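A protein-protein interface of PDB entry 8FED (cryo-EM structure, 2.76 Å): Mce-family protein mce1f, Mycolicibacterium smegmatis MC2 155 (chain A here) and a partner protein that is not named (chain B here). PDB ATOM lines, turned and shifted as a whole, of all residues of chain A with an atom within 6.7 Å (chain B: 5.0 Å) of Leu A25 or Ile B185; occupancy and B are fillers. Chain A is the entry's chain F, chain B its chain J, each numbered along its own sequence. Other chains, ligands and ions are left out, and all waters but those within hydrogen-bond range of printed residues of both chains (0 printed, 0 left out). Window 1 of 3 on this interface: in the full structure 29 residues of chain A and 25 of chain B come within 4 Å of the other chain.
O of Leu A25 sits at hydrogen-bond distance from N of Leu A30, 2.8 Å away.
Among the printed residues, merely in contact across the chains: Ala A21 with Met B183 (3.7 Å), Ala A21 with Leu B186 (3.3 Å), Leu A22 with Ala B182 (3.8 Å), Val A24 with Leu B186 (3.9 Å), Leu A25 with Ala B182 (3.9 Å), Leu A25 with Ile B185 (3.7 Å), Tyr A29 with Phe B189 (3.7 Å) and Tyr A29 with Met B190 (3.9 Å).
Printed residues of chain B within 4 Å of Ala A21: Met B183 (3.7 Å) and Leu B186 (3.3 Å). Of the printed residues of chain B, Val A24 touches Leu B186 (3.9 Å). Of chain B, only Ala B182 and Ile B185 come within 4 Å of Leu A25. Printed residues of chain B within 4 Å of Tyr A29: Phe B189 and Met B190. Tyr B181 touches none of the printed residues of chain A. Of the printed residues of chain A, Met B183 touches Ala A21 (3.7 Å). Printed residues of chain A within 4 Å of Leu B186: Ala A21 (3.3 Å) and Val A24 (3.9 Å). The nearest residue of chain B that does not touch Leu A25 is Leu B186 (4.04 Å). The nearest residue of chain A that does not touch Ile B185 is Leu A30 (5.5 Å).
Among the printed residues, 8 pairs touch across the chains. Among the printed residues, no Asp or Glu carboxylate lies within 4 Å of a Lys or Arg side-chain nitrogen of the other chain.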
ATOM      1  N   VAL A  20      28.460 -15.591  -6.694  1.00  0.00           N
ATOM      2  CA  VAL A  20      27.904 -14.241  -6.778  1.00  0.00           C
ATOM      3  C   VAL A  20      26.765 -14.198  -7.790  1.00  0.00           C
ATOM      4  O   VAL A  20      25.670 -13.697  -7.499  1.00  0.00           O
ATOM      5  CB  VAL A  20      29.007 -13.224  -7.124  1.00  0.00           C
ATOM      6  CG1 VAL A  20      28.397 -11.878  -7.477  1.00  0.00           C
ATOM      7  CG2 VAL A  20      29.971 -13.078  -5.959  1.00  0.00           C
ATOM      8  N   ALA A  21      26.999 -14.740  -8.990  1.00  0.00           N
ATOM      9  CA  ALA A  21      25.984 -14.702 -10.035  1.00  0.00           C
ATOM     10  C   ALA A  21      24.746 -15.495  -9.640  1.00  0.00           C
ATOM     11  O   ALA A  21      23.617 -15.042  -9.855  1.00  0.00           O
ATOM     12  CB  ALA A  21      26.561 -15.231 -11.347  1.00  0.00           C
ATOM     13  N   LEU A  22      24.938 -16.683  -9.060  1.00  0.00           N
ATOM     14  CA  LEU A  22      23.802 -17.516  -8.684  1.00  0.00           C
ATOM     15  C   LEU A  22      22.970 -16.859  -7.592  1.00  0.00           C
ATOM     16  O   LEU A  22      21.737 -16.866  -7.661  1.00  0.00           O
ATOM     17  CB  LEU A  22      24.293 -18.893  -8.240  1.00  0.00           C
ATOM     18  CG  LEU A  22      23.296 -20.048  -8.343  1.00  0.00           C
ATOM     19  CD1 LEU A  22      22.790 -20.194  -9.767  1.00  0.00           C
ATOM     20  CD2 LEU A  22      23.933 -21.341  -7.868  1.00  0.00           C
ATOM     21  N   VAL A  23      23.622 -16.272  -6.583  1.00  0.00           N
ATOM     22  CA  VAL A  23      22.882 -15.607  -5.514  1.00  0.00           C
ATOM     23  C   VAL A  23      22.127 -14.397  -6.053  1.00  0.00           C
ATOM     24  O   VAL A  23      20.955 -14.183  -5.715  1.00  0.00           O
ATOM     25  CB  VAL A  23      23.831 -15.227  -4.363  1.00  0.00           C
ATOM     26  CG1 VAL A  23      23.152 -14.269  -3.400  1.00  0.00           C
ATOM     27  CG2 VAL A  23      24.281 -16.476  -3.624  1.00  0.00           C
ATOM     28  N   VAL A  24      22.778 -13.588  -6.898  1.00  0.00           N
ATOM     29  CA  VAL A  24      22.117 -12.405  -7.446  1.00  0.00           C
ATOM     30  C   VAL A  24      20.917 -12.806  -8.295  1.00  0.00           C
ATOM     31  O   VAL A  24      19.835 -12.217  -8.182  1.00  0.00           O
ATOM     32  CB  VAL A  24      23.120 -11.548  -8.239  1.00  0.00           C
ATOM     33  CG1 VAL A  24      22.394 -10.486  -9.045  1.00  0.00           C
ATOM     34  CG2 VAL A  24      24.110 -10.893  -7.294  1.00  0.00           C
ATOM     35  N   LEU A  25      21.082 -13.821  -9.149  1.00  0.00           N
ATOM     36  CA  LEU A  25      19.974 -14.283  -9.977  1.00  0.00           C
ATOM     37  C   LEU A  25      18.837 -14.834  -9.126  1.00  0.00           C
ATOM     38  O   LEU A  25      17.661 -14.574  -9.406  1.00  0.00           O
ATOM     39  CB  LEU A  25      20.463 -15.342 -10.962  1.00  0.00           C
ATOM     40  CG  LEU A  25      19.406 -15.918 -11.904  1.00  0.00           C
ATOM     41  CD1 LEU A  25      18.913 -14.843 -12.853  1.00  0.00           C
ATOM     42  CD2 LEU A  25      19.950 -17.110 -12.671  1.00  0.00           C
ATOM     43  N   ALA A  26      19.167 -15.600  -8.083  1.00  0.00           N
ATOM     44  CA  ALA A  26      18.135 -16.203  -7.248  1.00  0.00           C
ATOM     45  C   ALA A  26      17.351 -15.148  -6.479  1.00  0.00           C
ATOM     46  O   ALA A  26      16.128 -15.261  -6.336  1.00  0.00           O
ATOM     47  CB  ALA A  26      18.765 -17.208  -6.286  1.00  0.00           C
ATOM     48  N   LEU A  27      18.029 -14.118  -5.977  1.00  0.00           N
ATOM     49  CA  LEU A  27      17.360 -13.151  -5.112  1.00  0.00           C
ATOM     50  C   LEU A  27      16.750 -11.992  -5.898  1.00  0.00           C
ATOM     51  O   LEU A  27      15.537 -11.774  -5.850  1.00  0.00           O
ATOM     52  CB  LEU A  27      18.339 -12.625  -4.056  1.00  0.00           C
ATOM     53  CG  LEU A  27      18.893 -13.663  -3.079  1.00  0.00           C
ATOM     54  CD1 LEU A  27      19.677 -12.984  -1.970  1.00  0.00           C
ATOM     55  CD2 LEU A  27      17.776 -14.518  -2.505  1.00  0.00           C
ATOM     56  N   PHE A  28      17.580 -11.240  -6.623  1.00  0.00           N
ATOM     57  CA  PHE A  28      17.131  -9.969  -7.176  1.00  0.00           C
ATOM     58  C   PHE A  28      16.348 -10.109  -8.476  1.00  0.00           C
ATOM     59  O   PHE A  28      15.658  -9.160  -8.863  1.00  0.00           O
ATOM     60  CB  PHE A  28      18.331  -9.046  -7.405  1.00  0.00           C
ATOM     61  CG  PHE A  28      19.024  -8.625  -6.141  1.00  0.00           C
ATOM     62  CD1 PHE A  28      19.955  -9.451  -5.532  1.00  0.00           C
ATOM     63  CD2 PHE A  28      18.747  -7.398  -5.561  1.00  0.00           C
ATOM     64  CE1 PHE A  28      20.593  -9.063  -4.370  1.00  0.00           C
ATOM     65  CE2 PHE A  28      19.382  -7.004  -4.400  1.00  0.00           C
ATOM     66  CZ  PHE A  28      20.307  -7.839  -3.804  1.00  0.00           C
ATOM     67  N   TYR A  29      16.430 -11.251  -9.158  1.00  0.00           N
ATOM     68  CA  TYR A  29      15.746 -11.417 -10.437  1.00  0.00           C
ATOM     69  C   TYR A  29      14.686 -12.509 -10.398  1.00  0.00           C
ATOM     70  O   TYR A  29      13.528 -12.243 -10.733  1.00  0.00           O
ATOM     71  CB  TYR A  29      16.769 -11.698 -11.545  1.00  0.00           C
ATOM     72  CG  TYR A  29      17.540 -10.475 -11.985  1.00  0.00           C
ATOM     73  CD1 TYR A  29      18.689 -10.075 -11.315  1.00  0.00           C
ATOM     74  CD2 TYR A  29      17.117  -9.717 -13.068  1.00  0.00           C
ATOM     75  CE1 TYR A  29      19.393  -8.958 -11.712  1.00  0.00           C
ATOM     76  CE2 TYR A  29      17.816  -8.599 -13.471  1.00  0.00           C
ATOM     77  CZ  TYR A  29      18.952  -8.225 -12.791  1.00  0.00           C
ATOM     78  OH  TYR A  29      19.652  -7.111 -13.190  1.00  0.00           O
ATOM     79  N   LEU A  30      15.042 -13.733 -10.006  1.00  0.00           N
ATOM     80  CA  LEU A  30      14.049 -14.799  -9.945  1.00  0.00           C
ATOM     81  C   LEU A  30      13.126 -14.664  -8.743  1.00  0.00           C
ATOM     82  O   LEU A  30      11.980 -15.126  -8.801  1.00  0.00           O
ATOM     83  CB  LEU A  30      14.736 -16.166  -9.918  1.00  0.00           C
ATOM     84  CG  LEU A  30      15.611 -16.524 -11.117  1.00  0.00           C
ATOM     85  CD1 LEU A  30      16.130 -17.944 -10.988  1.00  0.00           C
ATOM     86  CD2 LEU A  30      14.838 -16.345 -12.409  1.00  0.00           C
ATOM     87  N   ARG A  31      13.598 -14.036  -7.667  1.00  0.00           N
ATOM     88  CA  ARG A  31      12.863 -13.922  -6.407  1.00  0.00           C
ATOM     89  C   ARG A  31      12.425 -15.298  -5.903  1.00  0.00           C
ATOM     90  O   ARG A  31      11.240 -15.582  -5.725  1.00  0.00           O
ATOM     91  CB  ARG A  31      11.669 -12.974  -6.543  1.00  0.00           C
ATOM     92  CG  ARG A  31      12.048 -11.517  -6.730  1.00  0.00           C
ATOM     93  CD  ARG A  31      10.809 -10.643  -6.778  1.00  0.00           C
ATOM     94  NE  ARG A  31      11.137  -9.227  -6.889  1.00  0.00           N
ATOM     95  CZ  ARG A  31      10.239  -8.253  -6.902  1.00  0.00           C
ATOM     96  NH1 ARG A  31       8.944  -8.506  -6.812  1.00  0.00           N
ATOM     97  NH2 ARG A  31      10.649  -6.992  -7.009  1.00  0.00           N
ATOM     98  N   LEU A  32      13.419 -16.161  -5.702  1.00  0.00           N
ATOM     99  CA  LEU A  32      13.148 -17.506  -5.199  1.00  0.00           C
ATOM    100  C   LEU A  32      12.445 -17.542  -3.843  1.00  0.00           C
ATOM    101  O   LEU A  32      11.580 -18.417  -3.665  1.00  0.00           O
ATOM    102  CB  LEU A  32      14.449 -18.318  -5.150  1.00  0.00           C
ATOM    103  CG  LEU A  32      15.016 -18.767  -6.496  1.00  0.00           C
ATOM    104  CD1 LEU A  32      16.155 -19.748  -6.288  1.00  0.00           C
ATOM    105  CD2 LEU A  32      13.928 -19.388  -7.344  1.00  0.00           C
ATOM    106  N   ASN B 117      13.475 -13.779 -23.531  1.00  0.00           N
ATOM    107  CA  ASN B 117      14.707 -14.296 -22.951  1.00  0.00           C
ATOM    108  C   ASN B 117      14.530 -15.695 -22.387  1.00  0.00           C
ATOM    109  O   ASN B 117      15.510 -16.432 -22.266  1.00  0.00           O
ATOM    110  CB  ASN B 117      15.212 -13.355 -21.858  1.00  0.00           C
ATOM    111  CG  ASN B 117      15.934 -12.150 -22.417  1.00  0.00           C
ATOM    112  OD1 ASN B 117      16.849 -12.285 -23.226  1.00  0.00           O
ATOM    113  ND2 ASN B 117      15.524 -10.963 -21.992  1.00  0.00           N
ATOM    114  N   ILE B 118      13.308 -16.087 -22.038  1.00  0.00           N
ATOM    115  CA  ILE B 118      13.123 -17.423 -21.492  1.00  0.00           C
ATOM    116  C   ILE B 118      12.706 -18.368 -22.611  1.00  0.00           C
ATOM    117  O   ILE B 118      13.010 -19.567 -22.571  1.00  0.00           O
ATOM    118  CB  ILE B 118      12.101 -17.409 -20.343  1.00  0.00           C
ATOM    119  CG1 ILE B 118      12.547 -16.417 -19.272  1.00  0.00           C
ATOM    120  CG2 ILE B 118      11.988 -18.780 -19.714  1.00  0.00           C
ATOM    121  CD1 ILE B 118      13.910 -16.726 -18.694  1.00  0.00           C
ATOM    122  N   ALA B 122      17.675 -16.319 -25.174  1.00  0.00           N
ATOM    123  CA  ALA B 122      18.806 -16.663 -24.310  1.00  0.00           C
ATOM    124  C   ALA B 122      19.207 -18.131 -24.394  1.00  0.00           C
ATOM    125  O   ALA B 122      20.418 -18.401 -24.473  1.00  0.00           O
ATOM    126  CB  ALA B 122      18.525 -16.235 -22.867  1.00  0.00           C
ATOM    127  N   TYR B 181      25.121 -20.779 -17.603  1.00  0.00           N
ATOM    128  CA  TYR B 181      23.785 -20.351 -17.998  1.00  0.00           C
ATOM    129  C   TYR B 181      23.185 -19.381 -16.991  1.00  0.00           C
ATOM    130  O   TYR B 181      22.406 -18.504 -17.375  1.00  0.00           O
ATOM    131  CB  TYR B 181      22.865 -21.554 -18.189  1.00  0.00           C
ATOM    132  CG  TYR B 181      21.515 -21.170 -18.742  1.00  0.00           C
ATOM    133  CD1 TYR B 181      21.416 -20.401 -19.894  1.00  0.00           C
ATOM    134  CD2 TYR B 181      20.343 -21.567 -18.119  1.00  0.00           C
ATOM    135  CE1 TYR B 181      20.190 -20.038 -20.407  1.00  0.00           C
ATOM    136  CE2 TYR B 181      19.110 -21.210 -18.627  1.00  0.00           C
ATOM    137  CZ  TYR B 181      19.041 -20.447 -19.772  1.00  0.00           C
ATOM    138  OH  TYR B 181      17.817 -20.087 -20.284  1.00  0.00           O
ATOM    139  N   ALA B 182      23.532 -19.512 -15.707  1.00  0.00           N
ATOM    140  CA  ALA B 182      23.094 -18.521 -14.731  1.00  0.00           C
ATOM    141  C   ALA B 182      23.663 -17.144 -15.052  1.00  0.00           C
ATOM    142  O   ALA B 182      22.937 -16.142 -15.024  1.00  0.00           O
ATOM    143  CB  ALA B 182      23.497 -18.954 -13.322  1.00  0.00           C
ATOM    144  N   MET B 183      24.956 -17.079 -15.377  1.00  0.00           N
ATOM    145  CA  MET B 183      25.558 -15.809 -15.778  1.00  0.00           C
ATOM    146  C   MET B 183      24.933 -15.285 -17.063  1.00  0.00           C
ATOM    147  O   MET B 183      24.711 -14.078 -17.206  1.00  0.00           O
ATOM    148  CB  MET B 183      27.069 -15.964 -15.946  1.00  0.00           C
ATOM    149  CG  MET B 183      27.805 -16.368 -14.680  1.00  0.00           C
ATOM    150  SD  MET B 183      29.552 -16.702 -14.971  1.00  0.00           S
ATOM    151  CE  MET B 183      30.037 -17.395 -13.393  1.00  0.00           C
ATOM    152  N   ALA B 184      24.646 -16.181 -18.012  1.00  0.00           N
ATOM    153  CA  ALA B 184      24.032 -15.773 -19.272  1.00  0.00           C
ATOM    154  C   ALA B 184      22.660 -15.153 -19.044  1.00  0.00           C
ATOM    155  O   ALA B 184      22.347 -14.089 -19.589  1.00  0.00           O
ATOM    156  CB  ALA B 184      23.930 -16.976 -20.208  1.00  0.00           C
ATOM    157  N   ILE B 185      21.829 -15.809 -18.230  1.00  0.00           N
ATOM    158  CA  ILE B 185      20.496 -15.296 -17.926  1.00  0.00           C
ATOM    159  C   ILE B 185      20.587 -13.966 -17.190  1.00  0.00           C
ATOM    160  O   ILE B 185      19.865 -13.010 -17.510  1.00  0.00           O
ATOM    161  CB  ILE B 185      19.705 -16.341 -17.118  1.00  0.00           C
ATOM    162  CG1 ILE B 185      19.247 -17.475 -18.030  1.00  0.00           C
ATOM    163  CG2 ILE B 185      18.513 -15.712 -16.438  1.00  0.00           C
ATOM    164  CD1 ILE B 185      18.269 -17.036 -19.092  1.00  0.00           C
ATOM    165  N   LEU B 186      21.475 -13.882 -16.195  1.00  0.00           N
ATOM    166  CA  LEU B 186      21.629 -12.649 -15.430  1.00  0.00           C
ATOM    167  C   LEU B 186      22.043 -11.495 -16.333  1.00  0.00           C
ATOM    168  O   LEU B 186      21.482 -10.396 -16.253  1.00  0.00           O
ATOM    169  CB  LEU B 186      22.655 -12.862 -14.314  1.00  0.00           C
ATOM    170  CG  LEU B 186      22.597 -12.056 -13.013  1.00  0.00           C
ATOM    171  CD1 LEU B 186      23.620 -12.606 -12.041  1.00  0.00           C
ATOM    172  CD2 LEU B 186      22.827 -10.568 -13.216  1.00  0.00           C
ATOM    173  N   LEU B 187      23.016 -11.731 -17.216  1.00  0.00           N
ATOM    174  CA  LEU B 187      23.502 -10.661 -18.076  1.00  0.00           C
ATOM    175  C   LEU B 187      22.484 -10.286 -19.143  1.00  0.00           C
ATOM    176  O   LEU B 187      22.381  -9.109 -19.501  1.00  0.00           O
ATOM    177  CB  LEU B 187      24.836 -11.058 -18.703  1.00  0.00           C
ATOM    178  CG  LEU B 187      25.974 -11.079 -17.680  1.00  0.00           C
ATOM    179  CD1 LEU B 187      27.283 -11.472 -18.320  1.00  0.00           C
ATOM    180  CD2 LEU B 187      26.103  -9.727 -16.997  1.00  0.00           C
ATOM    181  N   SER B 188      21.718 -11.253 -19.653  1.00  0.00           N
ATOM    182  CA  SER B 188      20.658 -10.930 -20.604  1.00  0.00           C
ATOM    183  C   SER B 188      19.595 -10.048 -19.959  1.00  0.00           C
ATOM    184  O   SER B 188      19.188  -9.026 -20.529  1.00  0.00           O
ATOM    185  CB  SER B 188      20.039 -12.218 -21.146  1.00  0.00           C
ATOM    186  OG  SER B 188      19.032 -11.937 -22.098  1.00  0.00           O
ATOM    187  N   PHE B 189      19.142 -10.424 -18.755  1.00  0.00           N
ATOM    188  CA  PHE B 189      18.169  -9.605 -18.040  1.00  0.00           C
ATOM    189  C   PHE B 189      18.724  -8.219 -17.746  1.00  0.00           C
ATOM    190  O   PHE B 189      18.027  -7.211 -17.919  1.00  0.00           O
ATOM    191  CB  PHE B 189      17.750 -10.288 -16.738  1.00  0.00           C
ATOM    192  CG  PHE B 189      16.856 -11.479 -16.928  1.00  0.00           C
ATOM    193  CD1 PHE B 189      16.202 -11.691 -18.127  1.00  0.00           C
ATOM    194  CD2 PHE B 189      16.658 -12.379 -15.895  1.00  0.00           C
ATOM    195  CE1 PHE B 189      15.376 -12.785 -18.296  1.00  0.00           C
ATOM    196  CE2 PHE B 189      15.832 -13.470 -16.058  1.00  0.00           C
ATOM    197  CZ  PHE B 189      15.192 -13.675 -17.261  1.00  0.00           C
ATOM    198  N   MET B 190      19.979  -8.150 -17.292  1.00  0.00           N
ATOM    199  CA  MET B 190      20.586  -6.868 -16.958  1.00  0.00           C
ATOM    200  C   MET B 190      20.698  -5.973 -18.182  1.00  0.00           C
ATOM    201  O   MET B 190      20.409  -4.774 -18.109  1.00  0.00           O
ATOM    202  CB  MET B 190      21.960  -7.094 -16.327  1.00  0.00           C
ATOM    203  CG  MET B 190      22.721  -5.820 -16.012  1.00  0.00           C
ATOM    204  SD  MET B 190      24.345  -6.145 -15.303  1.00  0.00           S
ATOM    205  CE  MET B 190      23.892  -7.079 -13.844  1.00  0.00           C
ATOM    206  N   PHE B 224      16.721 -24.080 -17.709  1.00  0.00           N
ATOM    207  CA  PHE B 224      17.979 -24.628 -17.212  1.00  0.00           C
ATOM    208  C   PHE B 224      18.120 -26.100 -17.574  1.00  0.00           C
ATOM    209  O   PHE B 224      19.209 -26.550 -17.952  1.00  0.00           O
ATOM    210  CB  PHE B 224      18.081 -24.438 -15.700  1.00  0.00           C
ATOM    211  CG  PHE B 224      18.791 -23.180 -15.290  1.00  0.00           C
ATOM    212  CD1 PHE B 224      18.110 -21.979 -15.198  1.00  0.00           C
ATOM    213  CD2 PHE B 224      20.140 -23.202 -14.985  1.00  0.00           C
ATOM    214  CE1 PHE B 224      18.760 -20.824 -14.817  1.00  0.00           C
ATOM    215  CE2 PHE B 224      20.797 -22.050 -14.602  1.00  0.00           C
ATOM    216  CZ  PHE B 224      20.105 -20.859 -14.518  1.00  0.00           C
